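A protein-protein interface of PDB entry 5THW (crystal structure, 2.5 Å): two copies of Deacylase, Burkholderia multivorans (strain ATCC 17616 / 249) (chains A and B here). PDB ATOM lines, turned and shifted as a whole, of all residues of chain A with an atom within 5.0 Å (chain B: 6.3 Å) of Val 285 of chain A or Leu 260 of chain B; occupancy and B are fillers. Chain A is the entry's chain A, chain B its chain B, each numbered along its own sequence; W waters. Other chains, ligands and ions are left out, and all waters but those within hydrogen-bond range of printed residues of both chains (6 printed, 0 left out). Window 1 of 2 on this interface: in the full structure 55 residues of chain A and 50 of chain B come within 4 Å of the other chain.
O of Gly 286 of chain A is in hydrogen-bond range of N of Ser 294 of chain B (3.5 Å). SD of Met 287 of chain A is in hydrogen-bond range of NH2 of Arg 295 of chain B (3.5 Å).
O of Met 287 of chain A lies within hydrogen-bond range of N of Thr 305 of chain A, at 3.1 Å. The backbone NH of Leu 260 of chain B is in hydrogen-bond range of the side-chain carboxylate of Asp 258 of chain B (2.9 Å). The side-chain carboxylate (OD1) of Asp 258 of chain B is in hydrogen-bond range of the backbone NH (N) of Leu 261 of chain B (3.1 Å). The backbone NH (N) of Ala 259 of chain B sits at hydrogen-bond distance from the backbone carbonyl oxygen (O) of Pro 299 of chain B (3.0 Å). OG of Ser 264 of chain B is in hydrogen-bond range of O of Leu 260 of chain B (2.8 Å).
Among the printed residues, merely in contact across the chains: Val 267 of chain A with Ser 264 of chain B, Thr 305 of chain A with Arg 295 of chain B, Val 285 of chain A with Leu 260 of chain B, Val 285 of chain A with Pro 299 of chain B, Gly 286 of chain A with Val 297 of chain B, Gly 286 of chain A with Arg 295 of chain B, Gly 286 of chain A with Pro 299 of chain B, Gly 286 of chain A with Val 290 of chain B and Val 267 of chain A with Leu 261 of chain B.
Val 285 of chain A touches two residues of chain B. Leu 260 of chain B touches just one residue of chain A: Val 285. Of the printed residues of chain A, Val 297 of chain B touches Gly 286. Printed residues of chain B within 4 Å of Gly 286 of chain A: Val 290 (3.9 Å), Ser 294 (3.4 Å), Arg 295 (3.8 Å), Val 297 (3.5 Å) and Pro 299 (3.9 Å). Of the printed residues of chain A, Pro 299 of chain B touches Val 285 (3.5 Å) and Gly 286 (3.9 Å). Of the printed residues of chain A, Val 290 of chain B touches Gly 286 (3.9 Å). Of the printed residues of chain A, Arg 295 of chain B touches Gly 286 (3.8 Å), Met 287 (3.5 Å) and Thr 305 (3.3 Å). The nearest printed residue of chain B that does not touch Gly 286 of chain A is Leu 260 of chain B (4.9 Å).
Of the 12 printed residues of chain A, 5 touch a printed residue of chain B. Of the 21 printed residues of chain B, 8 touch a printed residue of chain A. Among the printed residues, 11 pairs touch across the chains.
1 position is printed for both chains. Of the 11 pairs that touch across the chains among the printed residues, none has its exchanged pair printed and touching as well.
Water W3 bridges the side-chain carboxylate (OD2) of Asp 258 of chain B (2.5 Å) and the backbone carbonyl oxygen (O) of Val 285 of chain A (2.9 Å). Water W4 lies within hydrogen-bond range of O of Arg 295 of chain B (2.6 Å), OG1 of Thr 305 of chain A (2.9 Å), N of Gly 286 of chain A (3.1 Å) and O of Thr 284 of chain A (3.1 Å). Water W1 bridges the guanidinium group (NH2) of Arg 295 of chain B (2.6 Å) and the side-chain sulfur (SD) of Met 287 of chain A (3.8 Å). Water W5 bridges the backbone carbonyl oxygen of Met 288 of chain A (2.7 Å) and the backbone NH of Val 290 of chain B (3.0 Å). Water W6 lies within hydrogen-bond range of the backbone carbonyl oxygen (O) of Gly 286 of chain A, the backbone NH (N) of Ser 294 of chain B and the backbone carbonyl oxygen (O) of Val 297 of chain B. Water W2 lies within hydrogen-bond range of the guanidinium group (NE) of Arg 295 of chain B (3.1 Å) and the side-chain sulfur (SD) of Met 287 of chain A (3.6 Å).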
ATOM      1  N   VAL A 266       0.313  21.689 -23.539  1.00  0.00           N
ATOM      2  CA  VAL A 266       1.233  20.562 -23.489  1.00  0.00           C
ATOM      3  C   VAL A 266       2.233  20.741 -22.350  1.00  0.00           C
ATOM      4  O   VAL A 266       2.597  19.773 -21.677  1.00  0.00           O
ATOM      5  CB  VAL A 266       1.919  20.361 -24.853  1.00  0.00           C
ATOM      6  CG1 VAL A 266       2.964  19.260 -24.766  1.00  0.00           C
ATOM      7  CG2 VAL A 266       0.875  19.985 -25.902  1.00  0.00           C
ATOM      8  N   VAL A 267       2.656  21.980 -22.080  1.00  0.00           N
ATOM      9  CA  VAL A 267       3.530  22.230 -20.933  1.00  0.00           C
ATOM     10  C   VAL A 267       2.884  21.708 -19.655  1.00  0.00           C
ATOM     11  O   VAL A 267       3.522  21.021 -18.848  1.00  0.00           O
ATOM     12  CB  VAL A 267       3.862  23.727 -20.818  1.00  0.00           C
ATOM     13  CG1 VAL A 267       4.559  24.015 -19.485  1.00  0.00           C
ATOM     14  CG2 VAL A 267       4.717  24.193 -22.000  1.00  0.00           C
ATOM     15  N   VAL A 270       2.700  17.868 -19.804  1.00  0.00           N
ATOM     16  CA  VAL A 270       4.009  17.302 -19.505  1.00  0.00           C
ATOM     17  C   VAL A 270       4.255  17.294 -18.002  1.00  0.00           C
ATOM     18  O   VAL A 270       4.686  16.283 -17.433  1.00  0.00           O
ATOM     19  CB  VAL A 270       5.096  18.084 -20.270  1.00  0.00           C
ATOM     20  CG1 VAL A 270       6.489  17.873 -19.654  1.00  0.00           C
ATOM     21  CG2 VAL A 270       5.078  17.672 -21.732  1.00  0.00           C
ATOM     22  N   ALA A 283       9.792  15.290 -15.813  1.00  0.00           N
ATOM     23  CA  ALA A 283       9.158  15.816 -17.015  1.00  0.00           C
ATOM     24  C   ALA A 283       9.312  17.334 -17.064  1.00  0.00           C
ATOM     25  O   ALA A 283       9.009  18.020 -16.082  1.00  0.00           O
ATOM     26  CB  ALA A 283       7.682  15.402 -17.061  1.00  0.00           C
ATOM     27  N   THR A 284       9.805  17.857 -18.190  1.00  0.00           N
ATOM     28  CA  THR A 284      10.102  19.283 -18.291  1.00  0.00           C
ATOM     29  C   THR A 284       9.961  19.774 -19.727  1.00  0.00           C
ATOM     30  O   THR A 284      10.304  19.061 -20.673  1.00  0.00           O
ATOM     31  CB  THR A 284      11.509  19.610 -17.773  1.00  0.00           C
ATOM     32  OG1 THR A 284      11.699  18.992 -16.497  1.00  0.00           O
ATOM     33  CG2 THR A 284      11.698  21.118 -17.627  1.00  0.00           C
ATOM     34  N   VAL A 285       9.438  20.989 -19.878  1.00  0.00           N
ATOM     35  CA  VAL A 285       9.513  21.741 -21.126  1.00  0.00           C
ATOM     36  C   VAL A 285      10.455  22.913 -20.881  1.00  0.00           C
ATOM     37  O   VAL A 285      10.115  23.855 -20.155  1.00  0.00           O
ATOM     38  CB  VAL A 285       8.138  22.221 -21.607  1.00  0.00           C
ATOM     39  CG1 VAL A 285       8.306  23.147 -22.814  1.00  0.00           C
ATOM     40  CG2 VAL A 285       7.235  21.031 -21.947  1.00  0.00           C
ATOM     41  N   GLY A 286      11.660  22.831 -21.438  1.00  0.00           N
ATOM     42  CA  GLY A 286      12.687  23.827 -21.204  1.00  0.00           C
ATOM     43  C   GLY A 286      12.869  24.858 -22.304  1.00  0.00           C
ATOM     44  O   GLY A 286      13.371  25.955 -22.046  1.00  0.00           O
ATOM     45  N   MET A 287      12.528  24.508 -23.545  1.00  0.00           N
ATOM     46  CA  MET A 287      12.803  25.365 -24.692  1.00  0.00           C
ATOM     47  C   MET A 287      11.522  25.608 -25.475  1.00  0.00           C
ATOM     48  O   MET A 287      10.791  24.661 -25.783  1.00  0.00           O
ATOM     49  CB  MET A 287      13.880  24.741 -25.606  1.00  0.00           C
ATOM     50  CG  MET A 287      14.279  25.599 -26.807  1.00  0.00           C
ATOM     51  SD  MET A 287      15.475  24.756 -27.882  1.00  0.00           S
ATOM     52  CE  MET A 287      15.804  26.025 -29.095  1.00  0.00           C
ATOM     53  N   MET A 288      11.260  26.873 -25.807  1.00  0.00           N
ATOM     54  CA  MET A 288      10.096  27.231 -26.605  1.00  0.00           C
ATOM     55  C   MET A 288      10.445  28.405 -27.516  1.00  0.00           C
ATOM     56  O   MET A 288      11.141  29.338 -27.100  1.00  0.00           O
ATOM     57  CB  MET A 288       8.904  27.575 -25.704  1.00  0.00           C
ATOM     58  CG  MET A 288       7.590  27.813 -26.452  1.00  0.00           C
ATOM     59  SD  MET A 288       6.176  28.042 -25.355  1.00  0.00           S
ATOM     60  CE  MET A 288       5.947  26.344 -24.799  1.00  0.00           C
ATOM     61  N   PHE A 304       8.713  23.601 -29.444  1.00  0.00           N
ATOM     62  CA  PHE A 304       9.095  23.427 -28.047  1.00  0.00           C
ATOM     63  C   PHE A 304       9.589  22.003 -27.832  1.00  0.00           C
ATOM     64  O   PHE A 304       9.387  21.118 -28.666  1.00  0.00           O
ATOM     65  CB  PHE A 304       7.939  23.785 -27.102  1.00  0.00           C
ATOM     66  CG  PHE A 304       6.746  22.885 -27.215  1.00  0.00           C
ATOM     67  CD1 PHE A 304       5.788  23.097 -28.197  1.00  0.00           C
ATOM     68  CD2 PHE A 304       6.553  21.851 -26.309  1.00  0.00           C
ATOM     69  CE1 PHE A 304       4.669  22.275 -28.288  1.00  0.00           C
ATOM     70  CE2 PHE A 304       5.438  21.030 -26.395  1.00  0.00           C
ATOM     71  CZ  PHE A 304       4.496  21.239 -27.387  1.00  0.00           C
ATOM     72  N   THR A 305      10.240  21.792 -26.691  1.00  0.00           N
ATOM     73  CA  THR A 305      10.874  20.517 -26.390  1.00  0.00           C
ATOM     74  C   THR A 305      10.228  19.863 -25.169  1.00  0.00           C
ATOM     75  O   THR A 305       9.605  20.526 -24.333  1.00  0.00           O
ATOM     76  CB  THR A 305      12.375  20.695 -26.157  1.00  0.00           C
ATOM     77  OG1 THR A 305      12.582  21.548 -25.026  1.00  0.00           O
ATOM     78  CG2 THR A 305      13.025  21.341 -27.391  1.00  0.00           C
ATOM     79  N   VAL A 306      10.372  18.539 -25.094  1.00  0.00           N
ATOM     80  CA  VAL A 306       9.897  17.732 -23.977  1.00  0.00           C
ATOM     81  C   VAL A 306      11.040  16.851 -23.487  1.00  0.00           C
ATOM     82  O   VAL A 306      11.768  16.256 -24.286  1.00  0.00           O
ATOM     83  CB  VAL A 306       8.671  16.877 -24.373  1.00  0.00           C
ATOM     84  CG1 VAL A 306       8.319  15.899 -23.268  1.00  0.00           C
ATOM     85  CG2 VAL A 306       7.458  17.777 -24.693  1.00  0.00           C
ATOM     86  N   PHE B 241       7.269  36.143 -14.998  1.00  0.00           N
ATOM     87  CA  PHE B 241       7.336  35.183 -13.904  1.00  0.00           C
ATOM     88  C   PHE B 241       8.798  34.856 -13.633  1.00  0.00           C
ATOM     89  O   PHE B 241       9.579  34.651 -14.570  1.00  0.00           O
ATOM     90  CB  PHE B 241       6.579  33.884 -14.226  1.00  0.00           C
ATOM     91  CG  PHE B 241       5.094  33.949 -13.975  1.00  0.00           C
ATOM     92  CD1 PHE B 241       4.575  34.749 -12.962  1.00  0.00           C
ATOM     93  CD2 PHE B 241       4.216  33.202 -14.748  1.00  0.00           C
ATOM     94  CE1 PHE B 241       3.213  34.807 -12.726  1.00  0.00           C
ATOM     95  CE2 PHE B 241       2.854  33.253 -14.518  1.00  0.00           C
ATOM     96  CZ  PHE B 241       2.349  34.057 -13.506  1.00  0.00           C
ATOM     97  N   ARG B 257      10.277  25.358  -9.194  1.00  0.00           N
ATOM     98  CA  ARG B 257       9.656  26.662  -9.413  1.00  0.00           C
ATOM     99  C   ARG B 257       9.822  26.999 -10.896  1.00  0.00           C
ATOM    100  O   ARG B 257      10.656  27.821 -11.282  1.00  0.00           O
ATOM    101  CB  ARG B 257      10.274  27.729  -8.466  1.00  0.00           C
ATOM    102  CG  ARG B 257      10.121  27.349  -6.989  1.00  0.00           C
ATOM    103  CD  ARG B 257      10.377  28.507  -6.030  1.00  0.00           C
ATOM    104  NE  ARG B 257      11.796  28.719  -5.747  1.00  0.00           N
ATOM    105  CZ  ARG B 257      12.469  29.818  -6.072  1.00  0.00           C
ATOM    106  NH1 ARG B 257      13.758  29.918  -5.771  1.00  0.00           N
ATOM    107  NH2 ARG B 257      11.854  30.823  -6.689  1.00  0.00           N
ATOM    108  N   ASP B 258       9.012  26.342 -11.725  1.00  0.00           N
ATOM    109  CA  ASP B 258       9.092  26.411 -13.180  1.00  0.00           C
ATOM    110  C   ASP B 258       8.320  27.634 -13.667  1.00  0.00           C
ATOM    111  O   ASP B 258       7.091  27.682 -13.566  1.00  0.00           O
ATOM    112  CB  ASP B 258       8.534  25.117 -13.770  1.00  0.00           C
ATOM    113  CG  ASP B 258       8.803  24.972 -15.265  1.00  0.00           C
ATOM    114  OD1 ASP B 258       8.773  25.989 -15.994  1.00  0.00           O
ATOM    115  OD2 ASP B 258       9.041  23.823 -15.713  1.00  0.00           O
ATOM    116  N   ALA B 259       9.033  28.612 -14.228  1.00  0.00           N
ATOM    117  CA  ALA B 259       8.379  29.847 -14.643  1.00  0.00           C
ATOM    118  C   ALA B 259       7.531  29.645 -15.893  1.00  0.00           C
ATOM    119  O   ALA B 259       6.570  30.391 -16.113  1.00  0.00           O
ATOM    120  CB  ALA B 259       9.418  30.945 -14.875  1.00  0.00           C
ATOM    121  N   LEU B 260       7.879  28.667 -16.734  1.00  0.00           N
ATOM    122  CA  LEU B 260       7.082  28.389 -17.927  1.00  0.00           C
ATOM    123  C   LEU B 260       5.795  27.648 -17.591  1.00  0.00           C
ATOM    124  O   LEU B 260       4.764  27.881 -18.235  1.00  0.00           O
ATOM    125  CB  LEU B 260       7.899  27.575 -18.937  1.00  0.00           C
ATOM    126  CG  LEU B 260       7.243  27.191 -20.268  1.00  0.00           C
ATOM    127  CD1 LEU B 260       6.811  28.427 -21.046  1.00  0.00           C
ATOM    128  CD2 LEU B 260       8.190  26.341 -21.096  1.00  0.00           C
ATOM    129  N   LEU B 261       5.825  26.787 -16.568  1.00  0.00           N
ATOM    130  CA  LEU B 261       4.595  26.155 -16.107  1.00  0.00           C
ATOM    131  C   LEU B 261       3.574  27.204 -15.691  1.00  0.00           C
ATOM    132  O   LEU B 261       2.391  27.105 -16.038  1.00  0.00           O
ATOM    133  CB  LEU B 261       4.891  25.209 -14.948  1.00  0.00           C
ATOM    134  CG  LEU B 261       3.702  24.416 -14.414  1.00  0.00           C
ATOM    135  CD1 LEU B 261       3.186  23.453 -15.487  1.00  0.00           C
ATOM    136  CD2 LEU B 261       4.101  23.680 -13.141  1.00  0.00           C
ATOM    137  N   GLY B 262       4.019  28.227 -14.961  1.00  0.00           N
ATOM    138  CA  GLY B 262       3.123  29.321 -14.624  1.00  0.00           C
ATOM    139  C   GLY B 262       2.661  30.090 -15.849  1.00  0.00           C
ATOM    140  O   GLY B 262       1.465  30.295 -16.054  1.00  0.00           O
ATOM    141  N   ALA B 263       3.608  30.496 -16.698  1.00  0.00           N
ATOM    142  CA  ALA B 263       3.258  31.268 -17.890  1.00  0.00           C
ATOM    143  C   ALA B 263       2.312  30.493 -18.802  1.00  0.00           C
ATOM    144  O   ALA B 263       1.429  31.082 -19.435  1.00  0.00           O
ATOM    145  CB  ALA B 263       4.525  31.667 -18.646  1.00  0.00           C
ATOM    146  N   SER B 264       2.492  29.172 -18.895  1.00  0.00           N
ATOM    147  CA  SER B 264       1.580  28.352 -19.688  1.00  0.00           C
ATOM    148  C   SER B 264       0.170  28.382 -19.112  1.00  0.00           C
ATOM    149  O   SER B 264      -0.813  28.426 -19.858  1.00  0.00           O
ATOM    150  CB  SER B 264       2.096  26.915 -19.769  1.00  0.00           C
ATOM    151  OG  SER B 264       3.351  26.873 -20.417  1.00  0.00           O
ATOM    152  N   ARG B 265       0.054  28.353 -17.782  1.00  0.00           N
ATOM    153  CA  ARG B 265      -1.262  28.383 -17.154  1.00  0.00           C
ATOM    154  C   ARG B 265      -1.928  29.746 -17.289  1.00  0.00           C
ATOM    155  O   ARG B 265      -3.163  29.827 -17.319  1.00  0.00           O
ATOM    156  CB  ARG B 265      -1.156  27.979 -15.681  1.00  0.00           C
ATOM    157  CG  ARG B 265      -0.884  26.504 -15.483  1.00  0.00           C
ATOM    158  CD  ARG B 265      -0.624  26.147 -14.026  1.00  0.00           C
ATOM    159  NE  ARG B 265      -0.385  24.714 -13.887  1.00  0.00           N
ATOM    160  CZ  ARG B 265       0.107  24.133 -12.797  1.00  0.00           C
ATOM    161  NH1 ARG B 265       0.417  24.862 -11.736  1.00  0.00           N
ATOM    162  NH2 ARG B 265       0.306  22.821 -12.778  1.00  0.00           N
ATOM    163  N   MET B 288       6.050  35.671 -26.018  1.00  0.00           N
ATOM    164  CA  MET B 288       6.613  34.971 -24.876  1.00  0.00           C
ATOM    165  C   MET B 288       8.101  34.781 -25.105  1.00  0.00           C
ATOM    166  O   MET B 288       8.525  34.469 -26.220  1.00  0.00           O
ATOM    167  CB  MET B 288       5.930  33.616 -24.646  1.00  0.00           C
ATOM    168  CG  MET B 288       6.396  32.904 -23.385  1.00  0.00           C
ATOM    169  SD  MET B 288       5.473  31.399 -23.040  1.00  0.00           S
ATOM    170  CE  MET B 288       3.928  32.066 -22.428  1.00  0.00           C
ATOM    171  N   VAL B 290      11.249  32.746 -23.108  1.00  0.00           N
ATOM    172  CA  VAL B 290      11.629  31.822 -22.041  1.00  0.00           C
ATOM    173  C   VAL B 290      13.123  31.941 -21.770  1.00  0.00           C
ATOM    174  O   VAL B 290      13.926  32.063 -22.701  1.00  0.00           O
ATOM    175  CB  VAL B 290      11.251  30.373 -22.401  1.00  0.00           C
ATOM    176  CG1 VAL B 290      11.744  29.413 -21.327  1.00  0.00           C
ATOM    177  CG2 VAL B 290       9.745  30.247 -22.559  1.00  0.00           C
ATOM    178  N   SER B 294      16.772  26.566 -22.468  1.00  0.00           N
ATOM    179  CA  SER B 294      17.565  25.369 -22.709  1.00  0.00           C
ATOM    180  C   SER B 294      16.703  24.148 -22.398  1.00  0.00           C
ATOM    181  O   SER B 294      16.082  24.079 -21.330  1.00  0.00           O
ATOM    182  CB  SER B 294      18.838  25.389 -21.856  1.00  0.00           C
ATOM    183  OG  SER B 294      19.648  24.257 -22.089  1.00  0.00           O
ATOM    184  N   ARG B 295      16.682  23.182 -23.325  1.00  0.00           N
ATOM    185  CA  ARG B 295      15.696  22.108 -23.258  1.00  0.00           C
ATOM    186  C   ARG B 295      15.812  21.277 -21.984  1.00  0.00           C
ATOM    187  O   ARG B 295      14.823  20.685 -21.540  1.00  0.00           O
ATOM    188  CB  ARG B 295      15.796  21.213 -24.495  1.00  0.00           C
ATOM    189  CG  ARG B 295      17.120  20.518 -24.706  1.00  0.00           C
ATOM    190  CD  ARG B 295      17.184  19.950 -26.114  1.00  0.00           C
ATOM    191  NE  ARG B 295      17.279  20.991 -27.138  1.00  0.00           N
ATOM    192  CZ  ARG B 295      16.770  20.886 -28.363  1.00  0.00           C
ATOM    193  NH1 ARG B 295      16.100  19.790 -28.713  1.00  0.00           N
ATOM    194  NH2 ARG B 295      16.925  21.875 -29.239  1.00  0.00           N
ATOM    195  N   VAL B 297      16.893  22.561 -18.974  1.00  0.00           N
ATOM    196  CA  VAL B 297      16.917  23.461 -17.824  1.00  0.00           C
ATOM    197  C   VAL B 297      15.486  23.882 -17.516  1.00  0.00           C
ATOM    198  O   VAL B 297      14.771  24.371 -18.399  1.00  0.00           O
ATOM    199  CB  VAL B 297      17.800  24.698 -18.066  1.00  0.00           C
ATOM    200  CG1 VAL B 297      17.752  25.633 -16.862  1.00  0.00           C
ATOM    201  CG2 VAL B 297      19.243  24.268 -18.332  1.00  0.00           C
ATOM    202  N   ILE B 298      15.067  23.689 -16.269  1.00  0.00           N
ATOM    203  CA  ILE B 298      13.789  24.275 -15.861  1.00  0.00           C
ATOM    204  C   ILE B 298      13.839  25.774 -16.120  1.00  0.00           C
ATOM    205  O   ILE B 298      14.802  26.445 -15.692  1.00  0.00           O
ATOM    206  CB  ILE B 298      13.512  23.987 -14.378  1.00  0.00           C
ATOM    207  CG1 ILE B 298      13.467  22.484 -14.131  1.00  0.00           C
ATOM    208  CG2 ILE B 298      12.224  24.656 -13.940  1.00  0.00           C
ATOM    209  CD1 ILE B 298      13.739  22.118 -12.705  1.00  0.00           C
ATOM    210  N   PRO B 299      12.874  26.351 -16.832  1.00  0.00           N
ATOM    211  CA  PRO B 299      12.940  27.791 -17.099  1.00  0.00           C
ATOM    212  C   PRO B 299      12.812  28.584 -15.803  1.00  0.00           C
ATOM    213  O   PRO B 299      11.922  28.334 -14.986  1.00  0.00           O
ATOM    214  CB  PRO B 299      11.762  28.032 -18.051  1.00  0.00           C
ATOM    215  CG  PRO B 299      11.558  26.708 -18.722  1.00  0.00           C
ATOM    216  CD  PRO B 299      11.829  25.693 -17.635  1.00  0.00           C
ATOM    217  N   GLY B 300      13.737  29.521 -15.609  1.00  0.00           N
ATOM    218  CA  GLY B 300      13.775  30.335 -14.410  1.00  0.00           C
ATOM    219  C   GLY B 300      13.112  31.691 -14.543  1.00  0.00           C
ATOM    220  O   GLY B 300      12.822  32.337 -13.534  1.00  0.00           O
ATOM    221  N   ARG B 301      12.885  32.148 -15.772  1.00  0.00           N
ATOM    222  CA  ARG B 301      12.207  33.417 -16.001  1.00  0.00           C
ATOM    223  C   ARG B 301      11.488  33.361 -17.343  1.00  0.00           C
ATOM    224  O   ARG B 301      12.029  32.841 -18.322  1.00  0.00           O
ATOM    225  CB  ARG B 301      13.197  34.587 -15.964  1.00  0.00           C
ATOM    226  CG  ARG B 301      12.559  35.965 -15.987  1.00  0.00           C
ATOM    227  CD  ARG B 301      13.607  37.073 -15.865  1.00  0.00           C
ATOM    228  NE  ARG B 301      14.247  37.397 -17.140  1.00  0.00           N
ATOM    229  CZ  ARG B 301      15.424  36.918 -17.540  1.00  0.00           C
ATOM    230  NH1 ARG B 301      16.110  36.081 -16.766  1.00  0.00           N
ATOM    231  NH2 ARG B 301      15.916  37.279 -18.719  1.00  0.00           N
ATOM    232  N   VAL B 302      10.265  33.878 -17.380  1.00  0.00           N
ATOM    233  CA  VAL B 302       9.495  33.947 -18.616  1.00  0.00           C
ATOM    234  C   VAL B 302       8.799  35.297 -18.662  1.00  0.00           C
ATOM    235  O   VAL B 302       8.055  35.651 -17.739  1.00  0.00           O
ATOM    236  CB  VAL B 302       8.460  32.813 -18.753  1.00  0.00           C
ATOM    237  CG1 VAL B 302       7.669  32.995 -20.042  1.00  0.00           C
ATOM    238  CG2 VAL B 302       9.142  31.453 -18.750  1.00  0.00           C
ATOM    239  N   LEU B 336       6.188  31.415  -7.671  1.00  0.00           N
ATOM    240  CA  LEU B 336       6.837  32.335  -8.589  1.00  0.00           C
ATOM    241  C   LEU B 336       6.740  33.767  -8.083  1.00  0.00           C
ATOM    242  O   LEU B 336       5.797  34.134  -7.378  1.00  0.00           O
ATOM    243  CB  LEU B 336       6.202  32.247  -9.976  1.00  0.00           C
ATOM    244  CG  LEU B 336       6.166  30.861 -10.602  1.00  0.00           C
ATOM    245  CD1 LEU B 336       5.346  30.923 -11.885  1.00  0.00           C
ATOM    246  CD2 LEU B 336       7.579  30.340 -10.859  1.00  0.00           C
HETATM  247  O   HOH W   1      18.804  23.675 -29.328  1.00  0.00           O
HETATM  248  O   HOH W   2      18.384  23.674 -26.073  1.00  0.00           O
HETATM  249  O   HOH W   3       8.311  23.099 -17.948  1.00  0.00           O
HETATM  250  O   HOH W   4      12.493  20.103 -22.537  1.00  0.00           O
HETATM  251  O   HOH W   5      11.054  31.709 -25.887  1.00  0.00           O
HETATM  252  O   HOH W   6      15.088  26.770 -20.071  1.00  0.00           O
